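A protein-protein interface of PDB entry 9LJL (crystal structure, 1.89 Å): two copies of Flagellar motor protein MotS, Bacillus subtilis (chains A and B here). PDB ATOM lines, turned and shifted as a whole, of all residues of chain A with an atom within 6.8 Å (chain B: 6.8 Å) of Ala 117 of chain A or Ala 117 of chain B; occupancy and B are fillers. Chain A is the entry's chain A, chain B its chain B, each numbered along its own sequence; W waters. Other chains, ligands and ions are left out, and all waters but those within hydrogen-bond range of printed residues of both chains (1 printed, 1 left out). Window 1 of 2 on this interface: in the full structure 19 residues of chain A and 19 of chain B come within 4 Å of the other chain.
The side-chain hydroxyl of Ser 121 of chain B sits at hydrogen-bond distance from the backbone carbonyl oxygen of Trp 113 of chain A, 3.1 Å away.
OG of Ser 121 of chain A is in hydrogen-bond range of O of Trp 113 of chain B (3.1 Å).
O of Ala 140 of chain A lies within hydrogen-bond range of N of Gly 142 of chain B (2.8 Å).
The backbone carbonyl oxygen (O) of Ala 140 of chain B lies within hydrogen-bond range of the backbone NH (N) of Gly 142 of chain A, at 2.8 Å.
The backbone NH (N) of Gly 97 of chain A sits at hydrogen-bond distance from the backbone carbonyl oxygen (O) of Val 141 of chain A (2.8 Å).
OG of Ser 116 of chain A sits at hydrogen-bond distance from O of Trp 113 of chain A (3.0 Å).
The backbone carbonyl oxygen of Val 95 of chain B lies within hydrogen-bond range of the backbone NH of Val 141 of chain B, 2.8 Å away.
The backbone NH of Gly 97 of chain B lies within hydrogen-bond range of the backbone carbonyl oxygen of Val 141 of chain B (2.8 Å).
The side-chain hydroxyl of Ser 116 of chain B is in hydrogen-bond range of the backbone carbonyl oxygen of Trp 113 of chain B (2.9 Å).
The side-chain hydroxyl (OG) of Ser 121 of chain B is in hydrogen-bond range of the backbone carbonyl oxygen (O) of Ala 117 of chain B, 2.9 Å away.
Among the printed residues, pairs that only touch across the chains: Glu 114 of chain A with Ser 121 of chain B, Glu 114 of chain A with Gly 122 of chain B, Ala 117 of chain A with Ala 117 of chain B, Ala 117 of chain A with Ser 121 of chain B, Ser 121 of chain A with Glu 114 of chain B, Ser 121 of chain A with Ala 117 of chain B, Gly 122 of chain A with Glu 114 of chain B, Ala 140 of chain A with Ala 140 of chain B, Ala 140 of chain A with Val 141 of chain B and Val 141 of chain A with Ala 140 of chain B.
Printed residues of chain B within 4 Å of Ala 117 of chain A: Ala 117 (3.7 Å) and Ser 121 (3.3 Å).
Of the printed residues of chain B, Glu 114 of chain A touches Ser 121 and Gly 122.
Of the printed residues of chain B, Gly 142 of chain A touches Ala 140.
Printed residues of chain A within 4 Å of Val 141 of chain B: Ala 140 (3.2 Å).
Of the printed residues of chain B, Val 141 of chain A touches Ala 140.
His 98 of chain A touches none of the printed residues of chain B.
The nearest residue of chain A that does not touch Ala 117 of chain B is Ala 140 of chain A (4.6 Å).
Along chain B the printed residues that touch a printed residue of chain A span positions 113 to 142.
Of the 21 printed residues of chain A, 8 touch a printed residue of chain B.
Hydrophobic or aromatic side chains of chain A that line the printed part of chain B: Trp 113, Ala 117, Ala 140 and Val 141.
Trp 113 of chain A touches Ser 121 of chain B, and with the chains exchanged Ser 121 of chain A touches Trp 113 of chain B.
Glu 114 of chain A touches Gly 122 of chain B, and with the chains exchanged Gly 122 of chain A touches Glu 114 of chain B.
Ala 140 of chain A touches Val 141 of chain B, and with the chains exchanged Val 141 of chain A touches Ala 140 of chain B.
Ala 140 of chain A touches Gly 142 of chain B, and with the chains exchanged Gly 142 of chain A touches Ala 140 of chain B.
Positions printed for both chains: 69, 95, 97, 98, 99, 112, 113, 114, 115, 116, 117, 118, 119, 120, 121, 122, 140, 141, 142, 143 and 144.
Water W1 lies within hydrogen-bond range of the backbone carbonyl oxygen (O) of Ala 69 of chain B (2.8 Å) and the side-chain carboxylate (OE2) of Glu 114 of chain A (3.3 Å).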
ATOM      1  N   ALA A  69      16.532 -11.617 -28.449  1.00  0.00           N
ATOM      2  CA  ALA A  69      15.915 -10.972 -27.294  1.00  0.00           C
ATOM      3  C   ALA A  69      14.530 -10.422 -27.611  1.00  0.00           C
ATOM      4  O   ALA A  69      14.025  -9.575 -26.869  1.00  0.00           O
ATOM      5  CB  ALA A  69      16.807  -9.855 -26.742  1.00  0.00           C
ATOM      6  N   VAL A  95      14.082  -6.875 -13.381  1.00  0.00           N
ATOM      7  CA  VAL A  95      14.124  -7.966 -14.350  1.00  0.00           C
ATOM      8  C   VAL A  95      15.577  -8.186 -14.753  1.00  0.00           C
ATOM      9  O   VAL A  95      16.230  -7.273 -15.270  1.00  0.00           O
ATOM     10  CB  VAL A  95      13.247  -7.663 -15.572  1.00  0.00           C
ATOM     11  CG1 VAL A  95      13.257  -8.840 -16.545  1.00  0.00           C
ATOM     12  CG2 VAL A  95      11.822  -7.349 -15.128  1.00  0.00           C
ATOM     13  N   GLY A  97      18.508 -10.412 -16.857  1.00  0.00           N
ATOM     14  CA  GLY A  97      18.831 -11.325 -17.943  1.00  0.00           C
ATOM     15  C   GLY A  97      20.134 -12.053 -17.660  1.00  0.00           C
ATOM     16  O   GLY A  97      21.100 -11.452 -17.188  1.00  0.00           O
ATOM     17  N   HIS A  98      20.152 -13.356 -17.956  1.00  0.00           N
ATOM     18  CA  HIS A  98      21.330 -14.198 -17.758  1.00  0.00           C
ATOM     19  C   HIS A  98      21.569 -15.060 -18.987  1.00  0.00           C
ATOM     20  O   HIS A  98      20.631 -15.654 -19.527  1.00  0.00           O
ATOM     21  CB  HIS A  98      21.173 -15.121 -16.546  1.00  0.00           C
ATOM     22  CG  HIS A  98      21.028 -14.394 -15.248  1.00  0.00           C
ATOM     23  ND1 HIS A  98      22.090 -14.161 -14.402  1.00  0.00           N
ATOM     24  CD2 HIS A  98      19.940 -13.850 -14.651  1.00  0.00           C
ATOM     25  CE1 HIS A  98      21.662 -13.501 -13.340  1.00  0.00           C
ATOM     26  NE2 HIS A  98      20.361 -13.303 -13.467  1.00  0.00           N
ATOM     27  N   THR A  99      22.825 -15.146 -19.411  1.00  0.00           N
ATOM     28  CA  THR A  99      23.218 -16.011 -20.516  1.00  0.00           C
ATOM     29  C   THR A  99      24.076 -17.149 -19.985  1.00  0.00           C
ATOM     30  O   THR A  99      24.588 -17.094 -18.863  1.00  0.00           O
ATOM     31  CB  THR A  99      23.999 -15.230 -21.578  1.00  0.00           C
ATOM     32  OG1 THR A  99      25.241 -14.775 -21.026  1.00  0.00           O
ATOM     33  CG2 THR A  99      23.202 -14.029 -22.044  1.00  0.00           C
ATOM     34  N   ASN A 112      27.637 -10.994 -24.659  1.00  0.00           N
ATOM     35  CA  ASN A 112      26.654 -11.538 -23.727  1.00  0.00           C
ATOM     36  C   ASN A 112      26.096 -10.478 -22.790  1.00  0.00           C
ATOM     37  O   ASN A 112      24.979 -10.645 -22.288  1.00  0.00           O
ATOM     38  CB  ASN A 112      27.271 -12.681 -22.921  1.00  0.00           C
ATOM     39  CG  ASN A 112      27.066 -14.036 -23.584  1.00  0.00           C
ATOM     40  OD1 ASN A 112      26.064 -14.259 -24.269  1.00  0.00           O
ATOM     41  ND2 ASN A 112      28.015 -14.944 -23.387  1.00  0.00           N
ATOM     42  N   TRP A 113      26.841  -9.396 -22.544  1.00  0.00           N
ATOM     43  CA  TRP A 113      26.294  -8.291 -21.764  1.00  0.00           C
ATOM     44  C   TRP A 113      25.105  -7.661 -22.476  1.00  0.00           C
ATOM     45  O   TRP A 113      24.038  -7.477 -21.879  1.00  0.00           O
ATOM     46  CB  TRP A 113      27.378  -7.243 -21.488  1.00  0.00           C
ATOM     47  CG  TRP A 113      28.405  -7.694 -20.493  1.00  0.00           C
ATOM     48  CD1 TRP A 113      29.675  -8.117 -20.756  1.00  0.00           C
ATOM     49  CD2 TRP A 113      28.242  -7.778 -19.070  1.00  0.00           C
ATOM     50  NE1 TRP A 113      30.315  -8.452 -19.587  1.00  0.00           N
ATOM     51  CE2 TRP A 113      29.453  -8.259 -18.538  1.00  0.00           C
ATOM     52  CE3 TRP A 113      27.186  -7.495 -18.196  1.00  0.00           C
ATOM     53  CZ2 TRP A 113      29.643  -8.458 -17.175  1.00  0.00           C
ATOM     54  CZ3 TRP A 113      27.377  -7.693 -16.840  1.00  0.00           C
ATOM     55  CH2 TRP A 113      28.591  -8.173 -16.344  1.00  0.00           C
ATOM     56  N   GLU A 114      25.264  -7.327 -23.762  1.00  0.00           N
ATOM     57  CA  GLU A 114      24.146  -6.738 -24.499  1.00  0.00           C
ATOM     58  C   GLU A 114      22.985  -7.711 -24.648  1.00  0.00           C
ATOM     59  O   GLU A 114      21.822  -7.304 -24.576  1.00  0.00           O
ATOM     60  CB  GLU A 114      24.593  -6.240 -25.875  1.00  0.00           C
ATOM     61  CG  GLU A 114      25.518  -5.032 -25.905  1.00  0.00           C
ATOM     62  CD  GLU A 114      26.987  -5.362 -25.760  1.00  0.00           C
ATOM     63  OE1 GLU A 114      27.327  -6.536 -25.511  1.00  0.00           O
ATOM     64  OE2 GLU A 114      27.807  -4.437 -25.952  1.00  0.00           O
ATOM     65  N   LEU A 115      23.266  -8.998 -24.867  1.00  0.00           N
ATOM     66  CA  LEU A 115      22.165  -9.945 -25.026  1.00  0.00           C
ATOM     67  C   LEU A 115      21.379 -10.089 -23.727  1.00  0.00           C
ATOM     68  O   LEU A 115      20.145 -10.097 -23.740  1.00  0.00           O
ATOM     69  CB  LEU A 115      22.681 -11.305 -25.498  1.00  0.00           C
ATOM     70  CG  LEU A 115      21.583 -12.363 -25.683  1.00  0.00           C
ATOM     71  CD1 LEU A 115      20.617 -11.931 -26.772  1.00  0.00           C
ATOM     72  CD2 LEU A 115      22.167 -13.733 -26.005  1.00  0.00           C
ATOM     73  N   SER A 116      22.079 -10.214 -22.595  1.00  0.00           N
ATOM     74  CA  SER A 116      21.382 -10.355 -21.318  1.00  0.00           C
ATOM     75  C   SER A 116      20.594  -9.096 -20.977  1.00  0.00           C
ATOM     76  O   SER A 116      19.477  -9.178 -20.444  1.00  0.00           O
ATOM     77  CB  SER A 116      22.377 -10.691 -20.203  1.00  0.00           C
ATOM     78  OG  SER A 116      23.185  -9.577 -19.851  1.00  0.00           O
ATOM     79  N   ALA A 117      21.158  -7.927 -21.285  1.00  0.00           N
ATOM     80  CA  ALA A 117      20.464  -6.670 -21.019  1.00  0.00           C
ATOM     81  C   ALA A 117      19.278  -6.477 -21.955  1.00  0.00           C
ATOM     82  O   ALA A 117      18.231  -5.958 -21.543  1.00  0.00           O
ATOM     83  CB  ALA A 117      21.442  -5.503 -21.148  1.00  0.00           C
ATOM     84  N   ALA A 118      19.429  -6.876 -23.222  1.00  0.00           N
ATOM     85  CA  ALA A 118      18.339  -6.754 -24.183  1.00  0.00           C
ATOM     86  C   ALA A 118      17.151  -7.631 -23.813  1.00  0.00           C
ATOM     87  O   ALA A 118      16.002  -7.247 -24.058  1.00  0.00           O
ATOM     88  CB  ALA A 118      18.832  -7.107 -25.590  1.00  0.00           C
ATOM     89  N   ARG A 119      17.401  -8.801 -23.220  1.00  0.00           N
ATOM     90  CA  ARG A 119      16.301  -9.680 -22.828  1.00  0.00           C
ATOM     91  C   ARG A 119      15.529  -9.107 -21.647  1.00  0.00           C
ATOM     92  O   ARG A 119      14.292  -9.142 -21.631  1.00  0.00           O
ATOM     93  CB  ARG A 119      16.841 -11.073 -22.499  1.00  0.00           C
ATOM     94  CG  ARG A 119      17.256 -11.822 -23.741  1.00  0.00           C
ATOM     95  CD  ARG A 119      17.830 -13.194 -23.461  1.00  0.00           C
ATOM     96  NE  ARG A 119      17.839 -13.965 -24.698  1.00  0.00           N
ATOM     97  CZ  ARG A 119      18.007 -15.277 -24.763  1.00  0.00           C
ATOM     98  NH1 ARG A 119      18.223 -16.001 -23.677  1.00  0.00           N
ATOM     99  NH2 ARG A 119      17.961 -15.878 -25.950  1.00  0.00           N
ATOM    100  N   ALA A 120      16.237  -8.581 -20.648  1.00  0.00           N
ATOM    101  CA  ALA A 120      15.555  -7.934 -19.534  1.00  0.00           C
ATOM    102  C   ALA A 120      14.778  -6.719 -20.013  1.00  0.00           C
ATOM    103  O   ALA A 120      13.623  -6.515 -19.624  1.00  0.00           O
ATOM    104  CB  ALA A 120      16.562  -7.541 -18.461  1.00  0.00           C
ATOM    105  N   SER A 121      15.399  -5.910 -20.876  1.00  0.00           N
ATOM    106  CA  SER A 121      14.740  -4.734 -21.434  1.00  0.00           C
ATOM    107  C   SER A 121      13.507  -5.114 -22.241  1.00  0.00           C
ATOM    108  O   SER A 121      12.469  -4.450 -22.146  1.00  0.00           O
ATOM    109  CB  SER A 121      15.727  -3.968 -22.313  1.00  0.00           C
ATOM    110  OG  SER A 121      16.717  -3.369 -21.513  1.00  0.00           O
ATOM    111  N   GLY A 122      13.607  -6.174 -23.049  1.00  0.00           N
ATOM    112  CA  GLY A 122      12.472  -6.586 -23.857  1.00  0.00           C
ATOM    113  C   GLY A 122      11.269  -6.987 -23.020  1.00  0.00           C
ATOM    114  O   GLY A 122      10.125  -6.665 -23.359  1.00  0.00           O
ATOM    115  N   ALA A 140      15.990  -2.632 -15.558  1.00  0.00           N
ATOM    116  CA  ALA A 140      16.525  -3.707 -16.387  1.00  0.00           C
ATOM    117  C   ALA A 140      17.959  -4.000 -15.969  1.00  0.00           C
ATOM    118  O   ALA A 140      18.766  -3.080 -15.818  1.00  0.00           O
ATOM    119  CB  ALA A 140      16.468  -3.331 -17.866  1.00  0.00           C
ATOM    120  N   VAL A 141      18.274  -5.274 -15.768  1.00  0.00           N
ATOM    121  CA  VAL A 141      19.600  -5.676 -15.312  1.00  0.00           C
ATOM    122  C   VAL A 141      20.121  -6.787 -16.213  1.00  0.00           C
ATOM    123  O   VAL A 141      19.413  -7.767 -16.471  1.00  0.00           O
ATOM    124  CB  VAL A 141      19.591  -6.132 -13.841  1.00  0.00           C
ATOM    125  CG1 VAL A 141      20.995  -6.484 -13.380  1.00  0.00           C
ATOM    126  CG2 VAL A 141      19.024  -5.024 -12.957  1.00  0.00           C
ATOM    127  N   GLY A 142      21.352  -6.632 -16.691  1.00  0.00           N
ATOM    128  CA  GLY A 142      22.044  -7.674 -17.434  1.00  0.00           C
ATOM    129  C   GLY A 142      23.251  -8.172 -16.655  1.00  0.00           C
ATOM    130  O   GLY A 142      24.060  -7.376 -16.167  1.00  0.00           O
ATOM    131  N   TYR A 143      23.353  -9.500 -16.542  1.00  0.00           N
ATOM    132  CA  TYR A 143      24.462 -10.149 -15.852  1.00  0.00           C
ATOM    133  C   TYR A 143      25.409 -10.891 -16.782  1.00  0.00           C
ATOM    134  O   TYR A 143      26.410 -11.438 -16.307  1.00  0.00           O
ATOM    135  CB  TYR A 143      23.921 -11.123 -14.797  1.00  0.00           C
ATOM    136  CG  TYR A 143      23.543 -10.471 -13.484  1.00  0.00           C
ATOM    137  CD1 TYR A 143      24.520 -10.131 -12.562  1.00  0.00           C
ATOM    138  CD2 TYR A 143      22.221 -10.167 -13.178  1.00  0.00           C
ATOM    139  CE1 TYR A 143      24.194  -9.543 -11.358  1.00  0.00           C
ATOM    140  CE2 TYR A 143      21.885  -9.567 -11.971  1.00  0.00           C
ATOM    141  CZ  TYR A 143      22.881  -9.257 -11.069  1.00  0.00           C
ATOM    142  OH  TYR A 143      22.580  -8.657  -9.866  1.00  0.00           O
ATOM    143  N   ALA A 144      25.128 -10.928 -18.084  1.00  0.00           N
ATOM    144  CA  ALA A 144      25.890 -11.752 -19.031  1.00  0.00           C
ATOM    145  C   ALA A 144      25.981 -13.156 -18.428  1.00  0.00           C
ATOM    146  O   ALA A 144      24.952 -13.684 -17.979  1.00  0.00           O
ATOM    147  CB  ALA A 144      27.224 -11.080 -19.340  1.00  0.00           C
ATOM    148  N   ALA B  69      24.587   2.579 -29.241  1.00  0.00           N
ATOM    149  CA  ALA B  69      25.213   2.045 -28.036  1.00  0.00           C
ATOM    150  C   ALA B  69      26.609   1.493 -28.297  1.00  0.00           C
ATOM    151  O   ALA B  69      27.155   0.779 -27.445  1.00  0.00           O
ATOM    152  CB  ALA B  69      24.328   0.963 -27.399  1.00  0.00           C
ATOM    153  N   VAL B  95      26.978  -0.151 -13.821  1.00  0.00           N
ATOM    154  CA  VAL B  95      26.936   0.825 -14.910  1.00  0.00           C
ATOM    155  C   VAL B  95      25.487   0.988 -15.349  1.00  0.00           C
ATOM    156  O   VAL B  95      24.845   0.013 -15.760  1.00  0.00           O
ATOM    157  CB  VAL B  95      27.831   0.405 -16.089  1.00  0.00           C
ATOM    158  CG1 VAL B  95      27.873   1.508 -17.139  1.00  0.00           C
ATOM    159  CG2 VAL B  95      29.239   0.094 -15.598  1.00  0.00           C
ATOM    160  N   GLY B  97      22.553   2.986 -17.698  1.00  0.00           N
ATOM    161  CA  GLY B  97      22.221   3.781 -18.868  1.00  0.00           C
ATOM    162  C   GLY B  97      20.904   4.508 -18.664  1.00  0.00           C
ATOM    163  O   GLY B  97      19.948   3.936 -18.145  1.00  0.00           O
ATOM    164  N   HIS B  98      20.868   5.776 -19.087  1.00  0.00           N
ATOM    165  CA  HIS B  98      19.699   6.634 -18.949  1.00  0.00           C
ATOM    166  C   HIS B  98      19.463   7.371 -20.258  1.00  0.00           C
ATOM    167  O   HIS B  98      20.409   7.884 -20.859  1.00  0.00           O
ATOM    168  CB  HIS B  98      19.887   7.684 -17.833  1.00  0.00           C
ATOM    169  CG  HIS B  98      20.064   7.106 -16.461  1.00  0.00           C
ATOM    170  ND1 HIS B  98      19.013   6.896 -15.596  1.00  0.00           N
ATOM    171  CD2 HIS B  98      21.179   6.721 -15.798  1.00  0.00           C
ATOM    172  CE1 HIS B  98      19.471   6.396 -14.462  1.00  0.00           C
ATOM    173  NE2 HIS B  98      20.785   6.288 -14.556  1.00  0.00           N
ATOM    174  N   THR B  99      18.206   7.448 -20.686  1.00  0.00           N
ATOM    175  CA  THR B  99      17.823   8.209 -21.870  1.00  0.00           C
ATOM    176  C   THR B  99      17.018   9.436 -21.464  1.00  0.00           C
ATOM    177  O   THR B  99      16.674   9.626 -20.294  1.00  0.00           O
ATOM    178  CB  THR B  99      16.983   7.358 -22.833  1.00  0.00           C
ATOM    179  OG1 THR B  99      15.729   7.039 -22.212  1.00  0.00           O
ATOM    180  CG2 THR B  99      17.711   6.067 -23.173  1.00  0.00           C
ATOM    181  N   ASN B 112      13.523   2.840 -25.448  1.00  0.00           N
ATOM    182  CA  ASN B 112      14.527   3.435 -24.574  1.00  0.00           C
ATOM    183  C   ASN B 112      14.996   2.468 -23.491  1.00  0.00           C
ATOM    184  O   ASN B 112      16.098   2.636 -22.962  1.00  0.00           O
ATOM    185  CB  ASN B 112      13.984   4.714 -23.935  1.00  0.00           C
ATOM    186  CG  ASN B 112      14.190   5.936 -24.815  1.00  0.00           C
ATOM    187  OD1 ASN B 112      15.204   6.056 -25.501  1.00  0.00           O
ATOM    188  ND2 ASN B 112      13.224   6.847 -24.798  1.00  0.00           N
ATOM    189  N   TRP B 113      14.191   1.467 -23.132  1.00  0.00           N
ATOM    190  CA  TRP B 113      14.704   0.432 -22.241  1.00  0.00           C
ATOM    191  C   TRP B 113      15.892  -0.272 -22.873  1.00  0.00           C
ATOM    192  O   TRP B 113      16.960  -0.382 -22.261  1.00  0.00           O
ATOM    193  CB  TRP B 113      13.607  -0.576 -21.890  1.00  0.00           C
ATOM    194  CG  TRP B 113      12.627  -0.037 -20.924  1.00  0.00           C
ATOM    195  CD1 TRP B 113      11.353   0.373 -21.191  1.00  0.00           C
ATOM    196  CD2 TRP B 113      12.842   0.194 -19.526  1.00  0.00           C
ATOM    197  NE1 TRP B 113      10.750   0.817 -20.038  1.00  0.00           N
ATOM    198  CE2 TRP B 113      11.644   0.724 -19.004  1.00  0.00           C
ATOM    199  CE3 TRP B 113      13.921  -0.016 -18.663  1.00  0.00           C
ATOM    200  CZ2 TRP B 113      11.502   1.060 -17.664  1.00  0.00           C
ATOM    201  CZ3 TRP B 113      13.779   0.318 -17.328  1.00  0.00           C
ATOM    202  CH2 TRP B 113      12.575   0.848 -16.840  1.00  0.00           C
ATOM    203  N   GLU B 114      15.729  -0.735 -24.115  1.00  0.00           N
ATOM    204  CA  GLU B 114      16.814  -1.432 -24.796  1.00  0.00           C
ATOM    205  C   GLU B 114      18.010  -0.516 -25.012  1.00  0.00           C
ATOM    206  O   GLU B 114      19.160  -0.936 -24.839  1.00  0.00           O
ATOM    207  CB  GLU B 114      16.339  -1.967 -26.147  1.00  0.00           C
ATOM    208  CG  GLU B 114      15.727  -3.347 -26.124  1.00  0.00           C
ATOM    209  CD  GLU B 114      14.216  -3.289 -26.082  1.00  0.00           C
ATOM    210  OE1 GLU B 114      13.674  -2.165 -25.987  1.00  0.00           O
ATOM    211  OE2 GLU B 114      13.573  -4.356 -26.178  1.00  0.00           O
ATOM    212  N   LEU B 115      17.765   0.728 -25.426  1.00  0.00           N
ATOM    213  CA  LEU B 115      18.883   1.624 -25.694  1.00  0.00           C
ATOM    214  C   LEU B 115      19.681   1.885 -24.425  1.00  0.00           C
ATOM    215  O   LEU B 115      20.915   1.843 -24.442  1.00  0.00           O
ATOM    216  CB  LEU B 115      18.392   2.940 -26.305  1.00  0.00           C
ATOM    217  CG  LEU B 115      19.484   3.995 -26.548  1.00  0.00           C
ATOM    218  CD1 LEU B 115      20.502   3.516 -27.590  1.00  0.00           C
ATOM    219  CD2 LEU B 115      18.869   5.313 -26.993  1.00  0.00           C
ATOM    220  N   SER B 116      18.992   2.148 -23.311  1.00  0.00           N
ATOM    221  CA  SER B 116      19.702   2.439 -22.068  1.00  0.00           C
ATOM    222  C   SER B 116      20.504   1.233 -21.594  1.00  0.00           C
ATOM    223  O   SER B 116      21.667   1.367 -21.197  1.00  0.00           O
ATOM    224  CB  SER B 116      18.715   2.901 -20.991  1.00  0.00           C
ATOM    225  OG  SER B 116      17.842   1.861 -20.567  1.00  0.00           O
ATOM    226  N   ALA B 117      19.904   0.042 -21.647  1.00  0.00           N
ATOM    227  CA  ALA B 117      20.597  -1.161 -21.198  1.00  0.00           C
ATOM    228  C   ALA B 117      21.760  -1.526 -22.115  1.00  0.00           C
ATOM    229  O   ALA B 117      22.780  -2.047 -21.646  1.00  0.00           O
ATOM    230  CB  ALA B 117      19.603  -2.322 -21.105  1.00  0.00           C
ATOM    231  N   ALA B 118      21.624  -1.282 -23.419  1.00  0.00           N
ATOM    232  CA  ALA B 118      22.704  -1.604 -24.345  1.00  0.00           C
ATOM    233  C   ALA B 118      23.881  -0.657 -24.168  1.00  0.00           C
ATOM    234  O   ALA B 118      25.031  -1.046 -24.385  1.00  0.00           O
ATOM    235  CB  ALA B 118      22.201  -1.549 -25.788  1.00  0.00           C
ATOM    236  N   ARG B 119      23.609   0.589 -23.782  1.00  0.00           N
ATOM    237  CA  ARG B 119      24.690   1.527 -23.510  1.00  0.00           C
ATOM    238  C   ARG B 119      25.472   1.119 -22.265  1.00  0.00           C
ATOM    239  O   ARG B 119      26.706   1.139 -22.270  1.00  0.00           O
ATOM    240  CB  ARG B 119      24.124   2.941 -23.376  1.00  0.00           C
ATOM    241  CG  ARG B 119      23.914   3.596 -24.743  1.00  0.00           C
ATOM    242  CD  ARG B 119      23.273   4.984 -24.683  1.00  0.00           C
ATOM    243  NE  ARG B 119      23.402   5.636 -25.985  1.00  0.00           N
ATOM    244  CZ  ARG B 119      23.219   6.928 -26.214  1.00  0.00           C
ATOM    245  NH1 ARG B 119      22.863   7.758 -25.250  1.00  0.00           N
ATOM    246  NH2 ARG B 119      23.415   7.403 -27.442  1.00  0.00           N
ATOM    247  N   ALA B 120      24.778   0.746 -21.189  1.00  0.00           N
ATOM    248  CA  ALA B 120      25.492   0.245 -20.019  1.00  0.00           C
ATOM    249  C   ALA B 120      26.318  -0.986 -20.381  1.00  0.00           C
ATOM    250  O   ALA B 120      27.465  -1.125 -19.941  1.00  0.00           O
ATOM    251  CB  ALA B 120      24.510  -0.061 -18.892  1.00  0.00           C
ATOM    252  N   SER B 121      25.772  -1.850 -21.241  1.00  0.00           N
ATOM    253  CA  SER B 121      26.464  -3.075 -21.641  1.00  0.00           C
ATOM    254  C   SER B 121      27.718  -2.788 -22.452  1.00  0.00           C
ATOM    255  O   SER B 121      28.749  -3.447 -22.259  1.00  0.00           O
ATOM    256  CB  SER B 121      25.519  -3.962 -22.449  1.00  0.00           C
ATOM    257  OG  SER B 121      24.465  -4.410 -21.643  1.00  0.00           O
ATOM    258  N   GLY B 122      27.639  -1.855 -23.404  1.00  0.00           N
ATOM    259  CA  GLY B 122      28.796  -1.576 -24.231  1.00  0.00           C
ATOM    260  C   GLY B 122      29.951  -1.037 -23.422  1.00  0.00           C
ATOM    261  O   GLY B 122      31.112  -1.339 -23.711  1.00  0.00           O
ATOM    262  N   ALA B 140      25.119  -4.573 -15.569  1.00  0.00           N
ATOM    263  CA  ALA B 140      24.573  -3.602 -16.508  1.00  0.00           C
ATOM    264  C   ALA B 140      23.155  -3.254 -16.088  1.00  0.00           C
ATOM    265  O   ALA B 140      22.347  -4.151 -15.825  1.00  0.00           O
ATOM    266  CB  ALA B 140      24.574  -4.174 -17.927  1.00  0.00           C
ATOM    267  N   VAL B 141      22.845  -1.962 -16.029  1.00  0.00           N
ATOM    268  CA  VAL B 141      21.530  -1.522 -15.577  1.00  0.00           C
ATOM    269  C   VAL B 141      20.966  -0.530 -16.586  1.00  0.00           C
ATOM    270  O   VAL B 141      21.664   0.398 -17.008  1.00  0.00           O
ATOM    271  CB  VAL B 141      21.592  -0.892 -14.173  1.00  0.00           C
ATOM    272  CG1 VAL B 141      20.245  -0.287 -13.810  1.00  0.00           C
ATOM    273  CG2 VAL B 141      22.028  -1.925 -13.129  1.00  0.00           C
ATOM    274  N   GLY B 142      19.712  -0.735 -16.985  1.00  0.00           N
ATOM    275  CA  GLY B 142      19.025   0.232 -17.825  1.00  0.00           C
ATOM    276  C   GLY B 142      17.813   0.834 -17.139  1.00  0.00           C
ATOM    277  O   GLY B 142      16.974   0.101 -16.597  1.00  0.00           O
ATOM    278  N   TYR B 143      17.707   2.168 -17.154  1.00  0.00           N
ATOM    279  CA  TYR B 143      16.605   2.880 -16.524  1.00  0.00           C
ATOM    280  C   TYR B 143      15.694   3.597 -17.507  1.00  0.00           C
ATOM    281  O   TYR B 143      14.737   4.246 -17.070  1.00  0.00           O
ATOM    282  CB  TYR B 143      17.134   3.907 -15.510  1.00  0.00           C
ATOM    283  CG  TYR B 143      17.406   3.345 -14.136  1.00  0.00           C
ATOM    284  CD1 TYR B 143      16.357   3.028 -13.283  1.00  0.00           C
ATOM    285  CD2 TYR B 143      18.705   3.153 -13.681  1.00  0.00           C
ATOM    286  CE1 TYR B 143      16.590   2.522 -12.020  1.00  0.00           C
ATOM    287  CE2 TYR B 143      18.949   2.656 -12.411  1.00  0.00           C
ATOM    288  CZ  TYR B 143      17.888   2.338 -11.588  1.00  0.00           C
ATOM    289  OH  TYR B 143      18.118   1.832 -10.326  1.00  0.00           O
ATOM    290  N   ALA B 144      15.964   3.508 -18.806  1.00  0.00           N
ATOM    291  CA  ALA B 144      15.220   4.238 -19.841  1.00  0.00           C
ATOM    292  C   ALA B 144      15.158   5.703 -19.407  1.00  0.00           C
ATOM    293  O   ALA B 144      16.194   6.264 -19.024  1.00  0.00           O
ATOM    294  CB  ALA B 144      13.875   3.565 -20.083  1.00  0.00           C
HETATM  295  O   HOH W   1      26.672  -1.948 -27.860  1.00  0.00           O
